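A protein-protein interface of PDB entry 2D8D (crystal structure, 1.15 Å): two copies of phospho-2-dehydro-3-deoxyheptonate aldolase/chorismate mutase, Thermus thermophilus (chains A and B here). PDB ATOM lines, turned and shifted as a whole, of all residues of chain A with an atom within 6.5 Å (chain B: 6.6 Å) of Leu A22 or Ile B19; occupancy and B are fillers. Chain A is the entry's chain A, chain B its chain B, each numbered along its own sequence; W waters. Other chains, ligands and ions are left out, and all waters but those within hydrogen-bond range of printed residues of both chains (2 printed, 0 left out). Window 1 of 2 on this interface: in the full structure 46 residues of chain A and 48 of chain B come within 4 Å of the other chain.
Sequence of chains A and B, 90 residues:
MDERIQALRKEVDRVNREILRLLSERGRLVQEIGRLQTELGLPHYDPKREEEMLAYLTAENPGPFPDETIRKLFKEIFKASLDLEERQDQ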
ATOM      1  N   ARG A  17     -32.860   4.203   2.347  1.00  0.00           N
ATOM      2  CA  ARG A  17     -33.553   4.705   1.175  1.00  0.00           C
ATOM      3  C   ARG A  17     -32.696   5.663   0.362  1.00  0.00           C
ATOM      4  O   ARG A  17     -32.777   5.677  -0.868  1.00  0.00           O
ATOM      5  CB  ARG A  17     -34.888   5.329   1.593  1.00  0.00           C
ATOM      6  CG  ARG A  17     -35.894   4.263   2.022  1.00  0.00           C
ATOM      7  CD  ARG A  17     -37.206   4.846   2.521  1.00  0.00           C
ATOM      8  NE  ARG A  17     -38.253   3.822   2.561  1.00  0.00           N
ATOM      9  CZ  ARG A  17     -38.803   3.330   3.666  1.00  0.00           C
ATOM     10  NH1 ARG A  17     -38.428   3.758   4.862  1.00  0.00           N
ATOM     11  NH2 ARG A  17     -39.736   2.393   3.568  1.00  0.00           N
ATOM     12  N   GLU A  18     -31.863   6.451   1.033  1.00  0.00           N
ATOM     13  CA  GLU A  18     -30.972   7.355   0.321  1.00  0.00           C
ATOM     14  C   GLU A  18     -29.944   6.533  -0.453  1.00  0.00           C
ATOM     15  O   GLU A  18     -29.603   6.860  -1.586  1.00  0.00           O
ATOM     16  CB  GLU A  18     -30.251   8.289   1.294  1.00  0.00           C
ATOM     17  CG  GLU A  18     -31.067   9.484   1.731  1.00  0.00           C
ATOM     18  CD  GLU A  18     -30.249  10.495   2.508  1.00  0.00           C
ATOM     19  OE1 GLU A  18     -29.184  10.906   2.007  1.00  0.00           O
ATOM     20  OE2 GLU A  18     -30.671  10.888   3.615  1.00  0.00           O
ATOM     21  N   ILE A  19     -29.450   5.465   0.163  1.00  0.00           N
ATOM     22  CA  ILE A  19     -28.475   4.603  -0.491  1.00  0.00           C
ATOM     23  C   ILE A  19     -29.108   3.954  -1.724  1.00  0.00           C
ATOM     24  O   ILE A  19     -28.473   3.860  -2.776  1.00  0.00           O
ATOM     25  CB  ILE A  19     -27.949   3.517   0.487  1.00  0.00           C
ATOM     26  CG1 ILE A  19     -27.120   4.185   1.592  1.00  0.00           C
ATOM     27  CG2 ILE A  19     -27.116   2.481  -0.265  1.00  0.00           C
ATOM     28  CD1 ILE A  19     -26.719   3.260   2.732  1.00  0.00           C
ATOM     29  N   LEU A  20     -30.361   3.521  -1.600  1.00  0.00           N
ATOM     30  CA  LEU A  20     -31.053   2.911  -2.733  1.00  0.00           C
ATOM     31  C   LEU A  20     -31.128   3.908  -3.893  1.00  0.00           C
ATOM     32  O   LEU A  20     -30.896   3.547  -5.049  1.00  0.00           O
ATOM     33  CB  LEU A  20     -32.467   2.471  -2.331  1.00  0.00           C
ATOM     34  CG  LEU A  20     -33.349   1.924  -3.464  1.00  0.00           C
ATOM     35  CD1 LEU A  20     -32.705   0.690  -4.089  1.00  0.00           C
ATOM     36  CD2 LEU A  20     -34.730   1.587  -2.919  1.00  0.00           C
ATOM     37  N   ARG A  21     -31.442   5.161  -3.583  1.00  0.00           N
ATOM     38  CA  ARG A  21     -31.538   6.193  -4.610  1.00  0.00           C
ATOM     39  C   ARG A  21     -30.186   6.421  -5.284  1.00  0.00           C
ATOM     40  O   ARG A  21     -30.107   6.515  -6.510  1.00  0.00           O
ATOM     41  CB  ARG A  21     -32.034   7.509  -4.000  1.00  0.00           C
ATOM     42  CG  ARG A  21     -32.100   8.660  -4.994  1.00  0.00           C
ATOM     43  CD  ARG A  21     -32.644   9.929  -4.360  1.00  0.00           C
ATOM     44  NE  ARG A  21     -32.788  11.002  -5.340  1.00  0.00           N
ATOM     45  CZ  ARG A  21     -33.273  12.208  -5.063  1.00  0.00           C
ATOM     46  NH1 ARG A  21     -33.662  12.499  -3.829  1.00  0.00           N
ATOM     47  NH2 ARG A  21     -33.369  13.123  -6.017  1.00  0.00           N
ATOM     48  N   LEU A  22     -29.127   6.517  -4.486  1.00  0.00           N
ATOM     49  CA  LEU A  22     -27.793   6.743  -5.034  1.00  0.00           C
ATOM     50  C   LEU A  22     -27.277   5.556  -5.838  1.00  0.00           C
ATOM     51  O   LEU A  22     -26.631   5.739  -6.868  1.00  0.00           O
ATOM     52  CB  LEU A  22     -26.812   7.110  -3.917  1.00  0.00           C
ATOM     53  CG  LEU A  22     -26.724   8.609  -3.587  1.00  0.00           C
ATOM     54  CD1 LEU A  22     -26.097   9.354  -4.760  1.00  0.00           C
ATOM     55  CD2 LEU A  22     -28.103   9.168  -3.272  1.00  0.00           C
ATOM     56  N   LEU A  23     -27.553   4.341  -5.381  1.00  0.00           N
ATOM     57  CA  LEU A  23     -27.127   3.162  -6.127  1.00  0.00           C
ATOM     58  C   LEU A  23     -27.820   3.164  -7.484  1.00  0.00           C
ATOM     59  O   LEU A  23     -27.205   2.881  -8.510  1.00  0.00           O
ATOM     60  CB  LEU A  23     -27.501   1.883  -5.377  1.00  0.00           C
ATOM     61  CG  LEU A  23     -26.672   1.512  -4.150  1.00  0.00           C
ATOM     62  CD1 LEU A  23     -27.316   0.326  -3.454  1.00  0.00           C
ATOM     63  CD2 LEU A  23     -25.246   1.173  -4.564  1.00  0.00           C
ATOM     64  N   SER A  24     -29.105   3.495  -7.488  1.00  0.00           N
ATOM     65  CA  SER A  24     -29.868   3.519  -8.726  1.00  0.00           C
ATOM     66  C   SER A  24     -29.341   4.599  -9.667  1.00  0.00           C
ATOM     67  O   SER A  24     -29.251   4.383 -10.877  1.00  0.00           O
ATOM     68  CB  SER A  24     -31.350   3.728  -8.417  1.00  0.00           C
ATOM     69  OG  SER A  24     -31.846   2.639  -7.652  1.00  0.00           O
ATOM     70  N   GLU A  25     -28.993   5.757  -9.114  1.00  0.00           N
ATOM     71  CA  GLU A  25     -28.440   6.835  -9.925  1.00  0.00           C
ATOM     72  C   GLU A  25     -27.125   6.367 -10.545  1.00  0.00           C
ATOM     73  O   GLU A  25     -26.861   6.619 -11.720  1.00  0.00           O
ATOM     74  CB  GLU A  25     -28.201   8.081  -9.071  1.00  0.00           C
ATOM     75  CG  GLU A  25     -27.460   9.200  -9.791  1.00  0.00           C
ATOM     76  CD  GLU A  25     -27.319  10.452  -8.942  1.00  0.00           C
ATOM     77  OE1 GLU A  25     -27.450  10.355  -7.705  1.00  0.00           O
ATOM     78  OE2 GLU A  25     -27.061  11.532  -9.514  1.00  0.00           O
ATOM     79  N   ARG A  26     -26.303   5.677  -9.755  1.00  0.00           N
ATOM     80  CA  ARG A  26     -25.032   5.183 -10.262  1.00  0.00           C
ATOM     81  C   ARG A  26     -25.286   4.212 -11.412  1.00  0.00           C
ATOM     82  O   ARG A  26     -24.565   4.216 -12.412  1.00  0.00           O
ATOM     83  CB  ARG A  26     -24.240   4.479  -9.156  1.00  0.00           C
ATOM     84  CG  ARG A  26     -22.784   4.290  -9.535  1.00  0.00           C
ATOM     85  CD  ARG A  26     -21.991   3.479  -8.515  1.00  0.00           C
ATOM     86  NE  ARG A  26     -20.574   3.479  -8.870  1.00  0.00           N
ATOM     87  CZ  ARG A  26     -20.032   2.721  -9.817  1.00  0.00           C
ATOM     88  NH1 ARG A  26     -20.778   1.871 -10.507  1.00  0.00           N
ATOM     89  NH2 ARG A  26     -18.748   2.860 -10.122  1.00  0.00           N
ATOM     90  N   GLY A  27     -26.314   3.381 -11.266  1.00  0.00           N
ATOM     91  CA  GLY A  27     -26.649   2.424 -12.306  1.00  0.00           C
ATOM     92  C   GLY A  27     -27.007   3.112 -13.611  1.00  0.00           C
ATOM     93  O   GLY A  27     -26.557   2.698 -14.686  1.00  0.00           O
ATOM     94  N   PHE A  74     -17.732  -1.684  -2.264  1.00  0.00           N
ATOM     95  CA  PHE A  74     -17.711  -1.062  -3.573  1.00  0.00           C
ATOM     96  C   PHE A  74     -17.392  -2.064  -4.676  1.00  0.00           C
ATOM     97  O   PHE A  74     -17.893  -1.926  -5.786  1.00  0.00           O
ATOM     98  CB  PHE A  74     -16.760   0.134  -3.581  1.00  0.00           C
ATOM     99  CG  PHE A  74     -17.409   1.403  -3.102  1.00  0.00           C
ATOM    100  CD1 PHE A  74     -18.247   2.131  -3.946  1.00  0.00           C
ATOM    101  CD2 PHE A  74     -17.224   1.850  -1.798  1.00  0.00           C
ATOM    102  CE1 PHE A  74     -18.891   3.284  -3.498  1.00  0.00           C
ATOM    103  CE2 PHE A  74     -17.867   3.004  -1.340  1.00  0.00           C
ATOM    104  CZ  PHE A  74     -18.699   3.720  -2.195  1.00  0.00           C
ATOM    105  N   ILE A  77     -20.625  -3.387  -5.540  1.00  0.00           N
ATOM    106  CA  ILE A  77     -21.410  -2.405  -6.277  1.00  0.00           C
ATOM    107  C   ILE A  77     -20.930  -2.356  -7.731  1.00  0.00           C
ATOM    108  O   ILE A  77     -21.737  -2.311  -8.657  1.00  0.00           O
ATOM    109  CB  ILE A  77     -21.285  -1.004  -5.628  1.00  0.00           C
ATOM    110  CG1 ILE A  77     -21.996  -1.001  -4.273  1.00  0.00           C
ATOM    111  CG2 ILE A  77     -21.869   0.066  -6.544  1.00  0.00           C
ATOM    112  CD1 ILE A  77     -21.749   0.250  -3.458  1.00  0.00           C
ATOM    113  N   ARG B  14     -18.797  11.625  -8.055  1.00  0.00           N
ATOM    114  CA  ARG B  14     -19.652  12.321  -7.102  1.00  0.00           C
ATOM    115  C   ARG B  14     -20.575  11.343  -6.385  1.00  0.00           C
ATOM    116  O   ARG B  14     -20.715  11.384  -5.162  1.00  0.00           O
ATOM    117  CB  ARG B  14     -20.493  13.385  -7.815  1.00  0.00           C
ATOM    118  CG  ARG B  14     -21.592  13.997  -6.943  1.00  0.00           C
ATOM    119  CD  ARG B  14     -22.441  14.994  -7.718  1.00  0.00           C
ATOM    120  NE  ARG B  14     -23.121  14.383  -8.859  1.00  0.00           N
ATOM    121  CZ  ARG B  14     -24.203  13.613  -8.784  1.00  0.00           C
ATOM    122  NH1 ARG B  14     -24.763  13.339  -7.612  1.00  0.00           N
ATOM    123  NH2 ARG B  14     -24.730  13.118  -9.894  1.00  0.00           N
ATOM    124  N   VAL B  15     -21.209  10.468  -7.157  1.00  0.00           N
ATOM    125  CA  VAL B  15     -22.119   9.491  -6.593  1.00  0.00           C
ATOM    126  C   VAL B  15     -21.373   8.508  -5.688  1.00  0.00           C
ATOM    127  O   VAL B  15     -21.864   8.160  -4.614  1.00  0.00           O
ATOM    128  CB  VAL B  15     -22.885   8.759  -7.716  1.00  0.00           C
ATOM    129  CG1 VAL B  15     -23.682   7.600  -7.146  1.00  0.00           C
ATOM    130  CG2 VAL B  15     -23.826   9.742  -8.413  1.00  0.00           C
ATOM    131  N   ASN B  16     -20.190   8.065  -6.109  1.00  0.00           N
ATOM    132  CA  ASN B  16     -19.390   7.157  -5.285  1.00  0.00           C
ATOM    133  C   ASN B  16     -19.111   7.799  -3.928  1.00  0.00           C
ATOM    134  O   ASN B  16     -19.227   7.153  -2.886  1.00  0.00           O
ATOM    135  CB  ASN B  16     -18.032   6.852  -5.923  1.00  0.00           C
ATOM    136  CG  ASN B  16     -18.102   5.833  -7.045  1.00  0.00           C
ATOM    137  OD1 ASN B  16     -19.077   5.097  -7.190  1.00  0.00           O
ATOM    138  ND2 ASN B  16     -17.037   5.771  -7.831  1.00  0.00           N
ATOM    139  N   ARG B  17     -18.710   9.067  -3.945  1.00  0.00           N
ATOM    140  CA  ARG B  17     -18.401   9.766  -2.707  1.00  0.00           C
ATOM    141  C   ARG B  17     -19.631   9.907  -1.823  1.00  0.00           C
ATOM    142  O   ARG B  17     -19.535   9.792  -0.603  1.00  0.00           O
ATOM    143  CB  ARG B  17     -17.763  11.125  -3.018  1.00  0.00           C
ATOM    144  CG  ARG B  17     -16.316  10.982  -3.486  1.00  0.00           C
ATOM    145  CD  ARG B  17     -15.640  12.321  -3.758  1.00  0.00           C
ATOM    146  NE  ARG B  17     -14.199  12.146  -3.934  1.00  0.00           N
ATOM    147  CZ  ARG B  17     -13.541  12.306  -5.079  1.00  0.00           C
ATOM    148  NH1 ARG B  17     -14.185  12.660  -6.183  1.00  0.00           N
ATOM    149  NH2 ARG B  17     -12.233  12.092  -5.121  1.00  0.00           N
ATOM    150  N   GLU B  18     -20.788  10.139  -2.433  1.00  0.00           N
ATOM    151  CA  GLU B  18     -22.018  10.247  -1.659  1.00  0.00           C
ATOM    152  C   GLU B  18     -22.356   8.895  -1.029  1.00  0.00           C
ATOM    153  O   GLU B  18     -22.799   8.829   0.117  1.00  0.00           O
ATOM    154  CB  GLU B  18     -23.174  10.712  -2.544  1.00  0.00           C
ATOM    155  CG  GLU B  18     -23.096  12.170  -2.968  1.00  0.00           C
ATOM    156  CD  GLU B  18     -24.314  12.620  -3.752  1.00  0.00           C
ATOM    157  OE1 GLU B  18     -25.445  12.337  -3.303  1.00  0.00           O
ATOM    158  OE2 GLU B  18     -24.144  13.265  -4.808  1.00  0.00           O
ATOM    159  N   ILE B  19     -22.158   7.814  -1.779  1.00  0.00           N
ATOM    160  CA  ILE B  19     -22.431   6.484  -1.244  1.00  0.00           C
ATOM    161  C   ILE B  19     -21.494   6.209  -0.064  1.00  0.00           C
ATOM    162  O   ILE B  19     -21.918   5.657   0.953  1.00  0.00           O
ATOM    163  CB  ILE B  19     -22.273   5.397  -2.341  1.00  0.00           C
ATOM    164  CG1 ILE B  19     -23.396   5.552  -3.375  1.00  0.00           C
ATOM    165  CG2 ILE B  19     -22.317   4.005  -1.724  1.00  0.00           C
ATOM    166  CD1 ILE B  19     -23.220   4.702  -4.615  1.00  0.00           C
ATOM    167  N   LEU B  20     -20.228   6.603  -0.186  1.00  0.00           N
ATOM    168  CA  LEU B  20     -19.283   6.400   0.910  1.00  0.00           C
ATOM    169  C   LEU B  20     -19.749   7.162   2.152  1.00  0.00           C
ATOM    170  O   LEU B  20     -19.693   6.647   3.271  1.00  0.00           O
ATOM    171  CB  LEU B  20     -17.883   6.873   0.507  1.00  0.00           C
ATOM    172  CG  LEU B  20     -16.812   6.863   1.607  1.00  0.00           C
ATOM    173  CD1 LEU B  20     -16.594   5.452   2.149  1.00  0.00           C
ATOM    174  CD2 LEU B  20     -15.516   7.425   1.036  1.00  0.00           C
ATOM    175  N   ARG B  21     -20.215   8.390   1.954  1.00  0.00           N
ATOM    176  CA  ARG B  21     -20.694   9.200   3.064  1.00  0.00           C
ATOM    177  C   ARG B  21     -21.919   8.559   3.716  1.00  0.00           C
ATOM    178  O   ARG B  21     -22.011   8.495   4.942  1.00  0.00           O
ATOM    179  CB  ARG B  21     -21.052  10.608   2.582  1.00  0.00           C
ATOM    180  CG  ARG B  21     -21.415  11.563   3.711  1.00  0.00           C
ATOM    181  CD  ARG B  21     -21.793  12.943   3.192  1.00  0.00           C
ATOM    182  NE  ARG B  21     -23.082  12.944   2.502  1.00  0.00           N
ATOM    183  CZ  ARG B  21     -24.248  12.718   3.099  1.00  0.00           C
ATOM    184  NH1 ARG B  21     -24.294  12.472   4.401  1.00  0.00           N
ATOM    185  NH2 ARG B  21     -25.371  12.734   2.392  1.00  0.00           N
ATOM    186  N   LEU B  22     -22.854   8.089   2.895  1.00  0.00           N
ATOM    187  CA  LEU B  22     -24.070   7.463   3.408  1.00  0.00           C
ATOM    188  C   LEU B  22     -23.788   6.143   4.109  1.00  0.00           C
ATOM    189  O   LEU B  22     -24.391   5.842   5.139  1.00  0.00           O
ATOM    190  CB  LEU B  22     -25.084   7.264   2.280  1.00  0.00           C
ATOM    191  CG  LEU B  22     -25.952   8.490   1.964  1.00  0.00           C
ATOM    192  CD1 LEU B  22     -26.898   8.751   3.126  1.00  0.00           C
ATOM    193  CD2 LEU B  22     -25.081   9.709   1.705  1.00  0.00           C
ATOM    194  N   LEU B  23     -22.883   5.346   3.551  1.00  0.00           N
ATOM    195  CA  LEU B  23     -22.524   4.083   4.176  1.00  0.00           C
ATOM    196  C   LEU B  23     -21.902   4.364   5.539  1.00  0.00           C
ATOM    197  O   LEU B  23     -22.188   3.670   6.517  1.00  0.00           O
ATOM    198  CB  LEU B  23     -21.522   3.319   3.312  1.00  0.00           C
ATOM    199  CG  LEU B  23     -22.051   2.627   2.059  1.00  0.00           C
ATOM    200  CD1 LEU B  23     -20.884   2.069   1.267  1.00  0.00           C
ATOM    201  CD2 LEU B  23     -23.019   1.513   2.442  1.00  0.00           C
ATOM    202  N   SER B  24     -21.049   5.383   5.603  1.00  0.00           N
ATOM    203  CA  SER B  24     -20.389   5.728   6.855  1.00  0.00           C
ATOM    204  C   SER B  24     -21.402   6.229   7.880  1.00  0.00           C
ATOM    205  O   SER B  24     -21.300   5.914   9.064  1.00  0.00           O
ATOM    206  CB  SER B  24     -19.294   6.771   6.607  1.00  0.00           C
ATOM    207  OG  SER B  24     -18.268   6.234   5.781  1.00  0.00           O
ATOM    208  N   PHE B  65     -31.188  -1.578 -11.421  1.00  0.00           N
ATOM    209  CA  PHE B  65     -30.760  -2.853 -10.854  1.00  0.00           C
ATOM    210  C   PHE B  65     -31.939  -3.772 -10.579  1.00  0.00           C
ATOM    211  O   PHE B  65     -33.004  -3.320 -10.156  1.00  0.00           O
ATOM    212  CB  PHE B  65     -29.997  -2.649  -9.545  1.00  0.00           C
ATOM    213  CG  PHE B  65     -28.667  -1.985  -9.714  1.00  0.00           C
ATOM    214  CD1 PHE B  65     -28.455  -0.699  -9.235  1.00  0.00           C
ATOM    215  CD2 PHE B  65     -27.623  -2.646 -10.353  1.00  0.00           C
ATOM    216  CE1 PHE B  65     -27.220  -0.076  -9.389  1.00  0.00           C
ATOM    217  CE2 PHE B  65     -26.384  -2.033 -10.514  1.00  0.00           C
ATOM    218  CZ  PHE B  65     -26.181  -0.745 -10.029  1.00  0.00           C
HETATM  219  O   HOH W   1     -27.222  12.324  -5.908  1.00  0.00           O
HETATM  220  O   HOH W   2     -31.892   0.035  -8.986  1.00  0.00           O
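The side-chain carboxylate (OE2) of Glu B18 lies within salt-bridge range of the guanidinium group (NH1) of Arg B14. The backbone carbonyl oxygen of Leu B20 sits at hydrogen-bond distance from the side-chain hydroxyl of Ser B24 (2.9 Å).
Printed residues of chain B that touch a printed residue of chain A: Arg B14, Val B15, Asn B16, Glu B18, Ile B19, Leu B20, Leu B22 and Phe B65. Hydrophobic or aromatic side chains of chain B within 4 Å of the printed part of chain A: Val B15, Ile B19, Leu B22 and Phe B65. Among the printed residues, 14 pairs touch across the chains.
Among the printed residues, pairs that only touch across the chains: Leu A23 with Phe B65, Glu A18 with Leu B22, Leu A22 with Glu B18, Leu A22 with Val B15, Phe A74 with Asn B16, Glu A25 with Val B15, Phe A74 with Ile B19, Arg A26 with Val B15, Ile A19 with Leu B22, Leu A22 with Ile B19, Phe A74 with Leu B20 and Gly A27 with Phe B65.
The side-chain carboxylate of Glu A25 is in salt-bridge range of the guanidinium group of Arg B14 (2.8 Å). NE of Arg A26 sits at hydrogen-bond distance from OD1 of Asn B16 (2.8 Å).
Of chain B, only Val B15 (3.5 Å), Glu B18 (3.4 Å) and Ile B19 (3.8 Å) come within 4 Å of Leu A22. Of chain A, only Leu A22 (3.8 Å) and Phe A74 (3.7 Å) come within 4 Å of Ile B19. Of the printed residues of chain B, Phe A74 touches Asn B16, Ile B19 and Leu B20. Printed residues of chain A within 4 Å of Leu B22: Glu A18 and Ile A19. Of the printed residues of chain A, Phe B65 touches Leu A23 and Gly A27. Of the printed residues of chain A, Leu B20 touches Phe A74 (3.8 Å). Of the printed residues of chain B, Leu A23 touches Phe B65. Ser A24 touches none of the printed residues of chain B. The nearest residue of chain B that does not touch Leu A22 is Arg B14 (5.1 Å).
Water W1 lies within hydrogen-bond range of OE1 of Glu A25 (2.7 Å), OE1 of Glu B18 (3.2 Å) and NH1 of Arg B14 (3.2 Å). Water W2 bridges the side-chain hydroxyl (OG) of Ser A24 (2.9 Å) and the backbone NH (N) of Phe B65 (3.0 Å).
Glu A18 touches Leu B22, and with the chains exchanged Leu A22 touches Glu B18. Ile A19 touches Leu B22, and with the chains exchanged Leu A22 touches Ile B19.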
